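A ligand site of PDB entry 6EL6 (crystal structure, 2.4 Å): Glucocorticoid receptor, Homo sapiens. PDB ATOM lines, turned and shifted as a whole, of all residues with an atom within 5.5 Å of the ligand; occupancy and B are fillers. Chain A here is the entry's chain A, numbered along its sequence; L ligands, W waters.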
ATOM      1  N   ILE A  62     -16.457  19.488 -21.447  1.00  0.00           N
ATOM      2  CA  ILE A  62     -15.585  18.311 -21.417  1.00  0.00           C
ATOM      3  C   ILE A  62     -14.408  18.471 -22.403  1.00  0.00           C
ATOM      4  O   ILE A  62     -13.256  18.267 -22.000  1.00  0.00           O
ATOM      5  CB  ILE A  62     -16.372  16.984 -21.604  1.00  0.00           C
ATOM      6  CG1 ILE A  62     -17.297  16.696 -20.379  1.00  0.00           C
ATOM      7  CG2 ILE A  62     -15.424  15.790 -21.855  1.00  0.00           C
ATOM      8  CD1 ILE A  62     -18.341  15.587 -20.530  1.00  0.00           C
ATOM      9  N   MET A  63     -14.699  18.867 -23.653  1.00  0.00           N
ATOM     10  CA  MET A  63     -13.661  19.057 -24.689  1.00  0.00           C
ATOM     11  C   MET A  63     -12.660  20.142 -24.306  1.00  0.00           C
ATOM     12  O   MET A  63     -11.462  19.944 -24.529  1.00  0.00           O
ATOM     13  CB  MET A  63     -14.275  19.303 -26.071  1.00  0.00           C
ATOM     14  CG  MET A  63     -14.777  18.050 -26.724  1.00  0.00           C
ATOM     15  SD  MET A  63     -15.485  18.402 -28.344  1.00  0.00           S
ATOM     16  CE  MET A  63     -15.685  16.754 -28.980  1.00  0.00           C
ATOM     17  N   LEU A  66     -10.466  18.865 -21.414  1.00  0.00           N
ATOM     18  CA  LEU A  66      -9.533  17.868 -21.956  1.00  0.00           C
ATOM     19  C   LEU A  66      -8.370  18.491 -22.722  1.00  0.00           C
ATOM     20  O   LEU A  66      -7.262  17.970 -22.644  1.00  0.00           O
ATOM     21  CB  LEU A  66     -10.239  16.778 -22.784  1.00  0.00           C
ATOM     22  CG  LEU A  66     -11.140  15.802 -22.011  1.00  0.00           C
ATOM     23  CD1 LEU A  66     -11.702  14.742 -22.921  1.00  0.00           C
ATOM     24  CD2 LEU A  66     -10.396  15.162 -20.842  1.00  0.00           C
ATOM     25  N   ASN A  67      -8.611  19.625 -23.426  1.00  0.00           N
ATOM     26  CA  ASN A  67      -7.568  20.373 -24.141  1.00  0.00           C
ATOM     27  C   ASN A  67      -6.589  20.949 -23.121  1.00  0.00           C
ATOM     28  O   ASN A  67      -5.388  20.762 -23.259  1.00  0.00           O
ATOM     29  CB  ASN A  67      -8.171  21.507 -24.971  1.00  0.00           C
ATOM     30  CG  ASN A  67      -8.807  21.097 -26.269  1.00  0.00           C
ATOM     31  OD1 ASN A  67      -8.590  19.997 -26.786  1.00  0.00           O
ATOM     32  ND2 ASN A  67      -9.586  21.991 -26.844  1.00  0.00           N
ATOM     33  N   LEU A  69      -6.027  19.948 -19.983  1.00  0.00           N
ATOM     34  CA  LEU A  69      -5.349  18.780 -19.410  1.00  0.00           C
ATOM     35  C   LEU A  69      -4.303  18.224 -20.404  1.00  0.00           C
ATOM     36  O   LEU A  69      -3.211  17.848 -19.988  1.00  0.00           O
ATOM     37  CB  LEU A  69      -6.399  17.703 -19.006  1.00  0.00           C
ATOM     38  CG  LEU A  69      -5.887  16.338 -18.428  1.00  0.00           C
ATOM     39  CD1 LEU A  69      -5.154  16.502 -17.079  1.00  0.00           C
ATOM     40  CD2 LEU A  69      -7.036  15.352 -18.282  1.00  0.00           C
ATOM     41  N   GLY A  70      -4.622  18.244 -21.706  1.00  0.00           N
ATOM     42  CA  GLY A  70      -3.745  17.799 -22.782  1.00  0.00           C
ATOM     43  C   GLY A  70      -2.424  18.556 -22.840  1.00  0.00           C
ATOM     44  O   GLY A  70      -1.380  17.968 -23.141  1.00  0.00           O
ATOM     45  N   GLN A  73      -0.382  17.327 -20.057  1.00  0.00           N
ATOM     46  CA  GLN A  73       0.109  15.982 -20.398  1.00  0.00           C
ATOM     47  C   GLN A  73       1.325  16.121 -21.310  1.00  0.00           C
ATOM     48  O   GLN A  73       2.294  15.378 -21.158  1.00  0.00           O
ATOM     49  CB  GLN A  73      -0.951  15.104 -21.114  1.00  0.00           C
ATOM     50  CG  GLN A  73      -2.288  14.864 -20.373  1.00  0.00           C
ATOM     51  CD  GLN A  73      -2.262  13.922 -19.184  1.00  0.00           C
ATOM     52  OE1 GLN A  73      -1.221  13.520 -18.643  1.00  0.00           O
ATOM     53  NE2 GLN A  73      -3.453  13.590 -18.702  1.00  0.00           N
ATOM     54  N   TRP A 103       3.135  13.804 -30.713  1.00  0.00           N
ATOM     55  CA  TRP A 103       2.286  14.277 -29.603  1.00  0.00           C
ATOM     56  C   TRP A 103       0.936  13.512 -29.434  1.00  0.00           C
ATOM     57  O   TRP A 103       0.704  12.948 -28.374  1.00  0.00           O
ATOM     58  CB  TRP A 103       2.064  15.789 -29.683  1.00  0.00           C
ATOM     59  CG  TRP A 103       1.138  16.233 -30.763  1.00  0.00           C
ATOM     60  CD1 TRP A 103       1.335  16.155 -32.113  1.00  0.00           C
ATOM     61  CD2 TRP A 103      -0.154  16.823 -30.585  1.00  0.00           C
ATOM     62  NE1 TRP A 103       0.259  16.691 -32.779  1.00  0.00           N
ATOM     63  CE2 TRP A 103      -0.670  17.113 -31.870  1.00  0.00           C
ATOM     64  CE3 TRP A 103      -0.917  17.194 -29.454  1.00  0.00           C
ATOM     65  CZ2 TRP A 103      -1.907  17.730 -32.053  1.00  0.00           C
ATOM     66  CZ3 TRP A 103      -2.145  17.790 -29.644  1.00  0.00           C
ATOM     67  CH2 TRP A 103      -2.634  18.058 -30.926  1.00  0.00           C
ATOM     68  N   MET A 104       0.115  13.446 -30.487  1.00  0.00           N
ATOM     69  CA  MET A 104      -1.185  12.754 -30.463  1.00  0.00           C
ATOM     70  C   MET A 104      -1.041  11.219 -30.405  1.00  0.00           C
ATOM     71  O   MET A 104      -1.876  10.586 -29.762  1.00  0.00           O
ATOM     72  CB  MET A 104      -2.079  13.219 -31.648  1.00  0.00           C
ATOM     73  CG  MET A 104      -3.554  12.801 -31.534  1.00  0.00           C
ATOM     74  SD  MET A 104      -4.361  13.094 -29.922  1.00  0.00           S
ATOM     75  CE  MET A 104      -4.498  14.885 -29.946  1.00  0.00           C
ATOM     76  N   LEU A 106       1.409   9.580 -28.859  1.00  0.00           N
ATOM     77  CA  LEU A 106       1.812   9.347 -27.472  1.00  0.00           C
ATOM     78  C   LEU A 106       0.602   9.422 -26.535  1.00  0.00           C
ATOM     79  O   LEU A 106       0.413   8.541 -25.704  1.00  0.00           O
ATOM     80  CB  LEU A 106       2.885  10.365 -27.032  1.00  0.00           C
ATOM     81  CG  LEU A 106       4.252  10.351 -27.751  1.00  0.00           C
ATOM     82  CD1 LEU A 106       5.137  11.476 -27.241  1.00  0.00           C
ATOM     83  CD2 LEU A 106       4.963   9.009 -27.604  1.00  0.00           C
ATOM     84  N   MET A 107      -0.236  10.453 -26.695  1.00  0.00           N
ATOM     85  CA  MET A 107      -1.390  10.671 -25.832  1.00  0.00           C
ATOM     86  C   MET A 107      -2.524   9.677 -26.055  1.00  0.00           C
ATOM     87  O   MET A 107      -3.147   9.270 -25.072  1.00  0.00           O
ATOM     88  CB  MET A 107      -1.882  12.113 -25.941  1.00  0.00           C
ATOM     89  CG  MET A 107      -0.935  13.112 -25.300  1.00  0.00           C
ATOM     90  SD  MET A 107      -1.744  14.680 -24.929  1.00  0.00           S
ATOM     91  CE  MET A 107      -2.207  15.223 -26.617  1.00  0.00           C
ATOM     92  N   ALA A 108      -2.778   9.268 -27.300  1.00  0.00           N
ATOM     93  CA  ALA A 108      -3.828   8.299 -27.605  1.00  0.00           C
ATOM     94  C   ALA A 108      -3.452   6.913 -27.064  1.00  0.00           C
ATOM     95  O   ALA A 108      -4.289   6.222 -26.487  1.00  0.00           O
ATOM     96  CB  ALA A 108      -4.088   8.236 -29.109  1.00  0.00           C
ATOM     97  N   ALA A 110      -1.094   6.231 -24.590  1.00  0.00           N
ATOM     98  CA  ALA A 110      -1.018   6.259 -23.125  1.00  0.00           C
ATOM     99  C   ALA A 110      -2.421   6.204 -22.507  1.00  0.00           C
ATOM    100  O   ALA A 110      -2.629   5.455 -21.556  1.00  0.00           O
ATOM    101  CB  ALA A 110      -0.221   7.472 -22.642  1.00  0.00           C
ATOM    102  N   LEU A 111      -3.387   6.925 -23.104  1.00  0.00           N
ATOM    103  CA  LEU A 111      -4.781   6.911 -22.669  1.00  0.00           C
ATOM    104  C   LEU A 111      -5.381   5.509 -22.871  1.00  0.00           C
ATOM    105  O   LEU A 111      -6.055   5.012 -21.968  1.00  0.00           O
ATOM    106  CB  LEU A 111      -5.612   7.981 -23.406  1.00  0.00           C
ATOM    107  CG  LEU A 111      -7.123   7.992 -23.151  1.00  0.00           C
ATOM    108  CD1 LEU A 111      -7.445   8.598 -21.825  1.00  0.00           C
ATOM    109  CD2 LEU A 111      -7.853   8.723 -24.246  1.00  0.00           C
ATOM    110  N   ARG A 114      -4.082   3.255 -20.123  1.00  0.00           N
ATOM    111  CA  ARG A 114      -4.745   3.636 -18.872  1.00  0.00           C
ATOM    112  C   ARG A 114      -6.202   3.160 -18.814  1.00  0.00           C
ATOM    113  O   ARG A 114      -6.649   2.697 -17.772  1.00  0.00           O
ATOM    114  CB  ARG A 114      -4.651   5.157 -18.620  1.00  0.00           C
ATOM    115  CG  ARG A 114      -4.595   5.511 -17.130  1.00  0.00           C
ATOM    116  CD  ARG A 114      -4.259   6.963 -16.855  1.00  0.00           C
ATOM    117  NE  ARG A 114      -2.847   7.274 -17.095  1.00  0.00           N
ATOM    118  CZ  ARG A 114      -2.297   8.463 -16.900  1.00  0.00           C
ATOM    119  NH1 ARG A 114      -1.013   8.659 -17.162  1.00  0.00           N
ATOM    120  NH2 ARG A 114      -3.029   9.482 -16.447  1.00  0.00           N
ATOM    121  N   CYS A 125     -10.434   6.666 -19.634  1.00  0.00           N
ATOM    122  CA  CYS A 125      -9.940   7.179 -18.372  1.00  0.00           C
ATOM    123  C   CYS A 125      -8.919   8.293 -18.604  1.00  0.00           C
ATOM    124  O   CYS A 125      -7.714   8.077 -18.483  1.00  0.00           O
ATOM    125  CB  CYS A 125      -9.375   6.060 -17.506  1.00  0.00           C
ATOM    126  SG  CYS A 125     -10.479   4.630 -17.355  1.00  0.00           S
ATOM    127  N   PHE A 126      -9.443   9.478 -18.983  1.00  0.00           N
ATOM    128  CA  PHE A 126      -8.646  10.683 -19.245  1.00  0.00           C
ATOM    129  C   PHE A 126      -7.935  11.155 -17.979  1.00  0.00           C
ATOM    130  O   PHE A 126      -6.757  11.476 -18.025  1.00  0.00           O
ATOM    131  CB  PHE A 126      -9.530  11.799 -19.843  1.00  0.00           C
ATOM    132  CG  PHE A 126      -9.744  11.701 -21.339  1.00  0.00           C
ATOM    133  CD1 PHE A 126      -8.809  12.230 -22.229  1.00  0.00           C
ATOM    134  CD2 PHE A 126     -10.887  11.097 -21.855  1.00  0.00           C
ATOM    135  CE1 PHE A 126      -9.013  12.146 -23.613  1.00  0.00           C
ATOM    136  CE2 PHE A 126     -11.096  11.030 -23.239  1.00  0.00           C
ATOM    137  CZ  PHE A 126     -10.157  11.549 -24.107  1.00  0.00           C
ATOM    138  N   ALA A 127      -8.638  11.136 -16.847  1.00  0.00           N
ATOM    139  CA  ALA A 127      -8.130  11.523 -15.529  1.00  0.00           C
ATOM    140  C   ALA A 127      -9.030  10.813 -14.494  1.00  0.00           C
ATOM    141  O   ALA A 127     -10.143  10.430 -14.860  1.00  0.00           O
ATOM    142  CB  ALA A 127      -8.214  13.027 -15.363  1.00  0.00           C
ATOM    143  N   MET A 142     -19.500  13.792 -29.207  1.00  0.00           N
ATOM    144  CA  MET A 142     -18.560  13.140 -28.289  1.00  0.00           C
ATOM    145  C   MET A 142     -18.045  11.812 -28.814  1.00  0.00           C
ATOM    146  O   MET A 142     -16.836  11.581 -28.773  1.00  0.00           O
ATOM    147  CB  MET A 142     -19.133  12.985 -26.879  1.00  0.00           C
ATOM    148  CG  MET A 142     -18.055  12.768 -25.819  1.00  0.00           C
ATOM    149  SD  MET A 142     -17.103  14.264 -25.472  1.00  0.00           S
ATOM    150  CE  MET A 142     -18.180  15.051 -24.365  1.00  0.00           C
ATOM    151  N   GLN A 145     -15.290  11.498 -31.870  1.00  0.00           N
ATOM    152  CA  GLN A 145     -13.880  11.664 -31.522  1.00  0.00           C
ATOM    153  C   GLN A 145     -13.384  10.533 -30.616  1.00  0.00           C
ATOM    154  O   GLN A 145     -12.291  10.011 -30.834  1.00  0.00           O
ATOM    155  CB  GLN A 145     -13.603  13.055 -30.918  1.00  0.00           C
ATOM    156  CG  GLN A 145     -12.115  13.405 -30.793  1.00  0.00           C
ATOM    157  CD  GLN A 145     -11.445  13.822 -32.089  1.00  0.00           C
ATOM    158  OE1 GLN A 145     -11.612  13.218 -33.142  1.00  0.00           O
ATOM    159  NE2 GLN A 145     -10.605  14.846 -32.018  1.00  0.00           N
ATOM    160  N   CYS A 146     -14.204  10.132 -29.615  1.00  0.00           N
ATOM    161  CA  CYS A 146     -13.924   9.083 -28.622  1.00  0.00           C
ATOM    162  C   CYS A 146     -13.660   7.704 -29.234  1.00  0.00           C
ATOM    163  O   CYS A 146     -12.893   6.927 -28.655  1.00  0.00           O
ATOM    164  CB  CYS A 146     -15.054   9.005 -27.591  1.00  0.00           C
ATOM    165  SG  CYS A 146     -15.071  10.345 -26.383  1.00  0.00           S
ATOM    166  N   MET A 149     -10.083   6.754 -29.940  1.00  0.00           N
ATOM    167  CA  MET A 149      -9.406   6.495 -28.689  1.00  0.00           C
ATOM    168  C   MET A 149      -9.818   5.108 -28.192  1.00  0.00           C
ATOM    169  O   MET A 149      -8.958   4.325 -27.774  1.00  0.00           O
ATOM    170  CB  MET A 149      -9.730   7.574 -27.632  1.00  0.00           C
ATOM    171  CG  MET A 149      -9.319   8.991 -27.994  1.00  0.00           C
ATOM    172  SD  MET A 149      -7.534   9.160 -28.110  1.00  0.00           S
ATOM    173  CE  MET A 149      -7.376  10.895 -27.767  1.00  0.00           C
ATOM    174  N   LEU A 235      -8.179  11.556 -35.523  1.00  0.00           N
ATOM    175  CA  LEU A 235      -8.318  12.451 -34.364  1.00  0.00           C
ATOM    176  C   LEU A 235      -7.929  13.898 -34.731  1.00  0.00           C
ATOM    177  O   LEU A 235      -8.580  14.832 -34.258  1.00  0.00           O
ATOM    178  CB  LEU A 235      -7.425  11.997 -33.187  1.00  0.00           C
ATOM    179  CG  LEU A 235      -7.809  10.748 -32.390  1.00  0.00           C
ATOM    180  CD1 LEU A 235      -6.609  10.220 -31.631  1.00  0.00           C
ATOM    181  CD2 LEU A 235      -8.937  11.022 -31.409  1.00  0.00           C
ATOM    182  N   TYR A 238     -10.711  16.417 -36.637  1.00  0.00           N
ATOM    183  CA  TYR A 238     -11.602  17.201 -35.781  1.00  0.00           C
ATOM    184  C   TYR A 238     -10.838  18.196 -34.897  1.00  0.00           C
ATOM    185  O   TYR A 238     -11.325  19.313 -34.683  1.00  0.00           O
ATOM    186  CB  TYR A 238     -12.556  16.309 -34.961  1.00  0.00           C
ATOM    187  CG  TYR A 238     -13.709  17.079 -34.354  1.00  0.00           C
ATOM    188  CD1 TYR A 238     -14.690  17.665 -35.166  1.00  0.00           C
ATOM    189  CD2 TYR A 238     -13.822  17.242 -32.984  1.00  0.00           C
ATOM    190  CE1 TYR A 238     -15.734  18.409 -34.620  1.00  0.00           C
ATOM    191  CE2 TYR A 238     -14.875  17.972 -32.418  1.00  0.00           C
ATOM    192  CZ  TYR A 238     -15.823  18.555 -33.238  1.00  0.00           C
ATOM    193  OH  TYR A 238     -16.866  19.281 -32.704  1.00  0.00           O
ATOM    194  N   CYS A 239      -9.651  17.820 -34.409  1.00  0.00           N
ATOM    195  CA  CYS A 239      -8.811  18.696 -33.588  1.00  0.00           C
ATOM    196  C   CYS A 239      -8.371  19.970 -34.335  1.00  0.00           C
ATOM    197  O   CYS A 239      -8.551  21.068 -33.813  1.00  0.00           O
ATOM    198  CB  CYS A 239      -7.620  17.924 -33.003  1.00  0.00           C
ATOM    199  SG  CYS A 239      -6.530  18.923 -31.949  1.00  0.00           S
ATOM    200  N   THR A 242     -11.483  22.348 -34.790  1.00  0.00           N
ATOM    201  CA  THR A 242     -11.898  23.062 -33.572  1.00  0.00           C
ATOM    202  C   THR A 242     -10.931  24.189 -33.222  1.00  0.00           C
ATOM    203  O   THR A 242     -11.358  25.213 -32.689  1.00  0.00           O
ATOM    204  CB  THR A 242     -12.161  22.130 -32.373  1.00  0.00           C
ATOM    205  OG1 THR A 242     -10.932  21.540 -31.950  1.00  0.00           O
ATOM    206  CG2 THR A 242     -13.184  21.079 -32.660  1.00  0.00           C
ATOM    207  N   PHE A 252      -7.611  26.047 -26.483  1.00  0.00           N
ATOM    208  CA  PHE A 252      -6.452  25.169 -26.405  1.00  0.00           C
ATOM    209  C   PHE A 252      -5.386  25.896 -25.607  1.00  0.00           C
ATOM    210  O   PHE A 252      -5.229  27.114 -25.781  1.00  0.00           O
ATOM    211  CB  PHE A 252      -5.900  24.833 -27.796  1.00  0.00           C
ATOM    212  CG  PHE A 252      -6.758  23.888 -28.589  1.00  0.00           C
ATOM    213  CD1 PHE A 252      -7.846  24.346 -29.324  1.00  0.00           C
ATOM    214  CD2 PHE A 252      -6.442  22.533 -28.653  1.00  0.00           C
ATOM    215  CE1 PHE A 252      -8.631  23.465 -30.062  1.00  0.00           C
ATOM    216  CE2 PHE A 252      -7.225  21.658 -29.408  1.00  0.00           C
ATOM    217  CZ  PHE A 252      -8.316  22.128 -30.113  1.00  0.00           C
ATOM    218  N   LEU A 256      -0.468  23.124 -26.548  1.00  0.00           N
ATOM    219  CA  LEU A 256      -1.185  22.485 -27.646  1.00  0.00           C
ATOM    220  C   LEU A 256      -1.302  23.407 -28.840  1.00  0.00           C
ATOM    221  O   LEU A 256      -1.048  22.960 -29.955  1.00  0.00           O
ATOM    222  CB  LEU A 256      -2.558  21.917 -27.246  1.00  0.00           C
ATOM    223  CG  LEU A 256      -2.580  20.799 -26.194  1.00  0.00           C
ATOM    224  CD1 LEU A 256      -3.932  20.180 -26.115  1.00  0.00           C
ATOM    225  CD2 LEU A 256      -1.528  19.723 -26.476  1.00  0.00           C
HETATM  226  C1  LIG L   1      -5.992  17.898 -28.188  1.00  0.00           C
HETATM  227  C2  LIG L   1      -7.242  17.072 -28.256  1.00  0.00           C
HETATM  228  C3  LIG L   1      -8.962  14.336 -27.618  1.00  0.00           C
HETATM  229  C4  LIG L   1     -10.185  13.726 -27.601  1.00  0.00           C
HETATM  230  C5  LIG L   1     -11.216  14.354 -26.927  1.00  0.00           C
HETATM  231  C6  LIG L   1      -9.888  16.110 -26.343  1.00  0.00           C
HETATM  232  C7  LIG L   1     -13.506  14.508 -26.652  1.00  0.00           C
HETATM  233  C8  LIG L   1      -6.133  14.724 -25.707  1.00  0.00           C
HETATM  234  C9  LIG L   1      -5.739  13.399 -25.727  1.00  0.00           C
HETATM  235  C10 LIG L   1      -5.928  14.712 -23.360  1.00  0.00           C
HETATM  236  C11 LIG L   1      -6.223  15.419 -24.514  1.00  0.00           C
HETATM  237  C12 LIG L   1      -5.913  15.025 -21.980  1.00  0.00           C
HETATM  238  N1  LIG L   1      -5.306  13.022 -22.104  1.00  0.00           N
HETATM  239  C13 LIG L   1      -4.652  11.854 -21.634  1.00  0.00           C
HETATM  240  C14 LIG L   1      -3.447   9.618 -20.631  1.00  0.00           C
HETATM  241  C15 LIG L   1      -9.310  17.458 -29.498  1.00  0.00           C
HETATM  242  C16 LIG L   1     -10.511  18.310 -29.512  1.00  0.00           C
HETATM  243  C17 LIG L   1     -11.383  18.366 -30.727  1.00  0.00           C
HETATM  244  C18 LIG L   1      -7.460  16.258 -26.986  1.00  0.00           C
HETATM  245  C19 LIG L   1      -8.782  15.553 -26.978  1.00  0.00           C
HETATM  246  N2  LIG L   1     -11.100  15.540 -26.296  1.00  0.00           N
HETATM  247  O1  LIG L   1     -12.427  13.642 -26.951  1.00  0.00           O
HETATM  248  O2  LIG L   1      -6.381  15.301 -26.945  1.00  0.00           O
HETATM  249  C20 LIG L   1      -5.433  12.676 -24.596  1.00  0.00           C
HETATM  250  C21 LIG L   1      -5.537  13.378 -23.416  1.00  0.00           C
HETATM  251  N3  LIG L   1      -5.543  14.002 -21.224  1.00  0.00           N
HETATM  252  C22 LIG L   1      -3.528  11.362 -22.267  1.00  0.00           C
HETATM  253  C23 LIG L   1      -2.927  10.223 -21.752  1.00  0.00           C
HETATM  254  C24 LIG L   1      -4.571  10.110 -19.999  1.00  0.00           C
HETATM  255  C25 LIG L   1      -5.168  11.243 -20.522  1.00  0.00           C
HETATM  256  F1  LIG L   1      -2.859   8.522 -20.140  1.00  0.00           F
HETATM  257  N4  LIG L   1      -8.361  17.924 -28.611  1.00  0.00           N
HETATM  258  O3  LIG L   1      -9.216  16.442 -30.185  1.00  0.00           O
HETATM  259  C26 LIG L   1     -11.869  17.681 -29.481  1.00  0.00           C
HETATM  260  O   HOH W   1       0.194  11.151 -22.091  1.00  0.00           O
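A nitrogen (N4) of the ligand lies within hydrogen-bond range of the side-chain amide oxygen of Asn 67 (2.8 Å). The side-chain amide nitrogen (NE2) of Gln 145 lies within hydrogen-bond range of an oxygen (O3) of the ligand, at 2.8 Å. A nitrogen (N3) of the ligand sits at hydrogen-bond distance from the side-chain amide nitrogen of Gln 73 (3.3 Å).
The backbone carbonyl oxygen of Met 142 is in hydrogen-bond range of the side-chain sulfur of Cys 146, at 3.2 Å. NE2 of Gln 145 is in hydrogen-bond range of O of Leu 235, 3.0 Å away. OG1 of Thr 242 lies within hydrogen-bond range of O of Cys 239 (3.1 Å).
O of Ala 110 sits close to F1 of the ligand. F1 of the ligand lies close to N of Leu 111 (3.4 Å). NE of Arg 114 sits close to F1 of the ligand (3.3 Å). Merely in contact with the ligand: Met 63, Leu 66, Leu 69, Gly 70, Met 104, Met 107, Phe 126, Met 142, Met 149, Tyr 238, Cys 239, Thr 242, Phe 252 and Leu 256.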
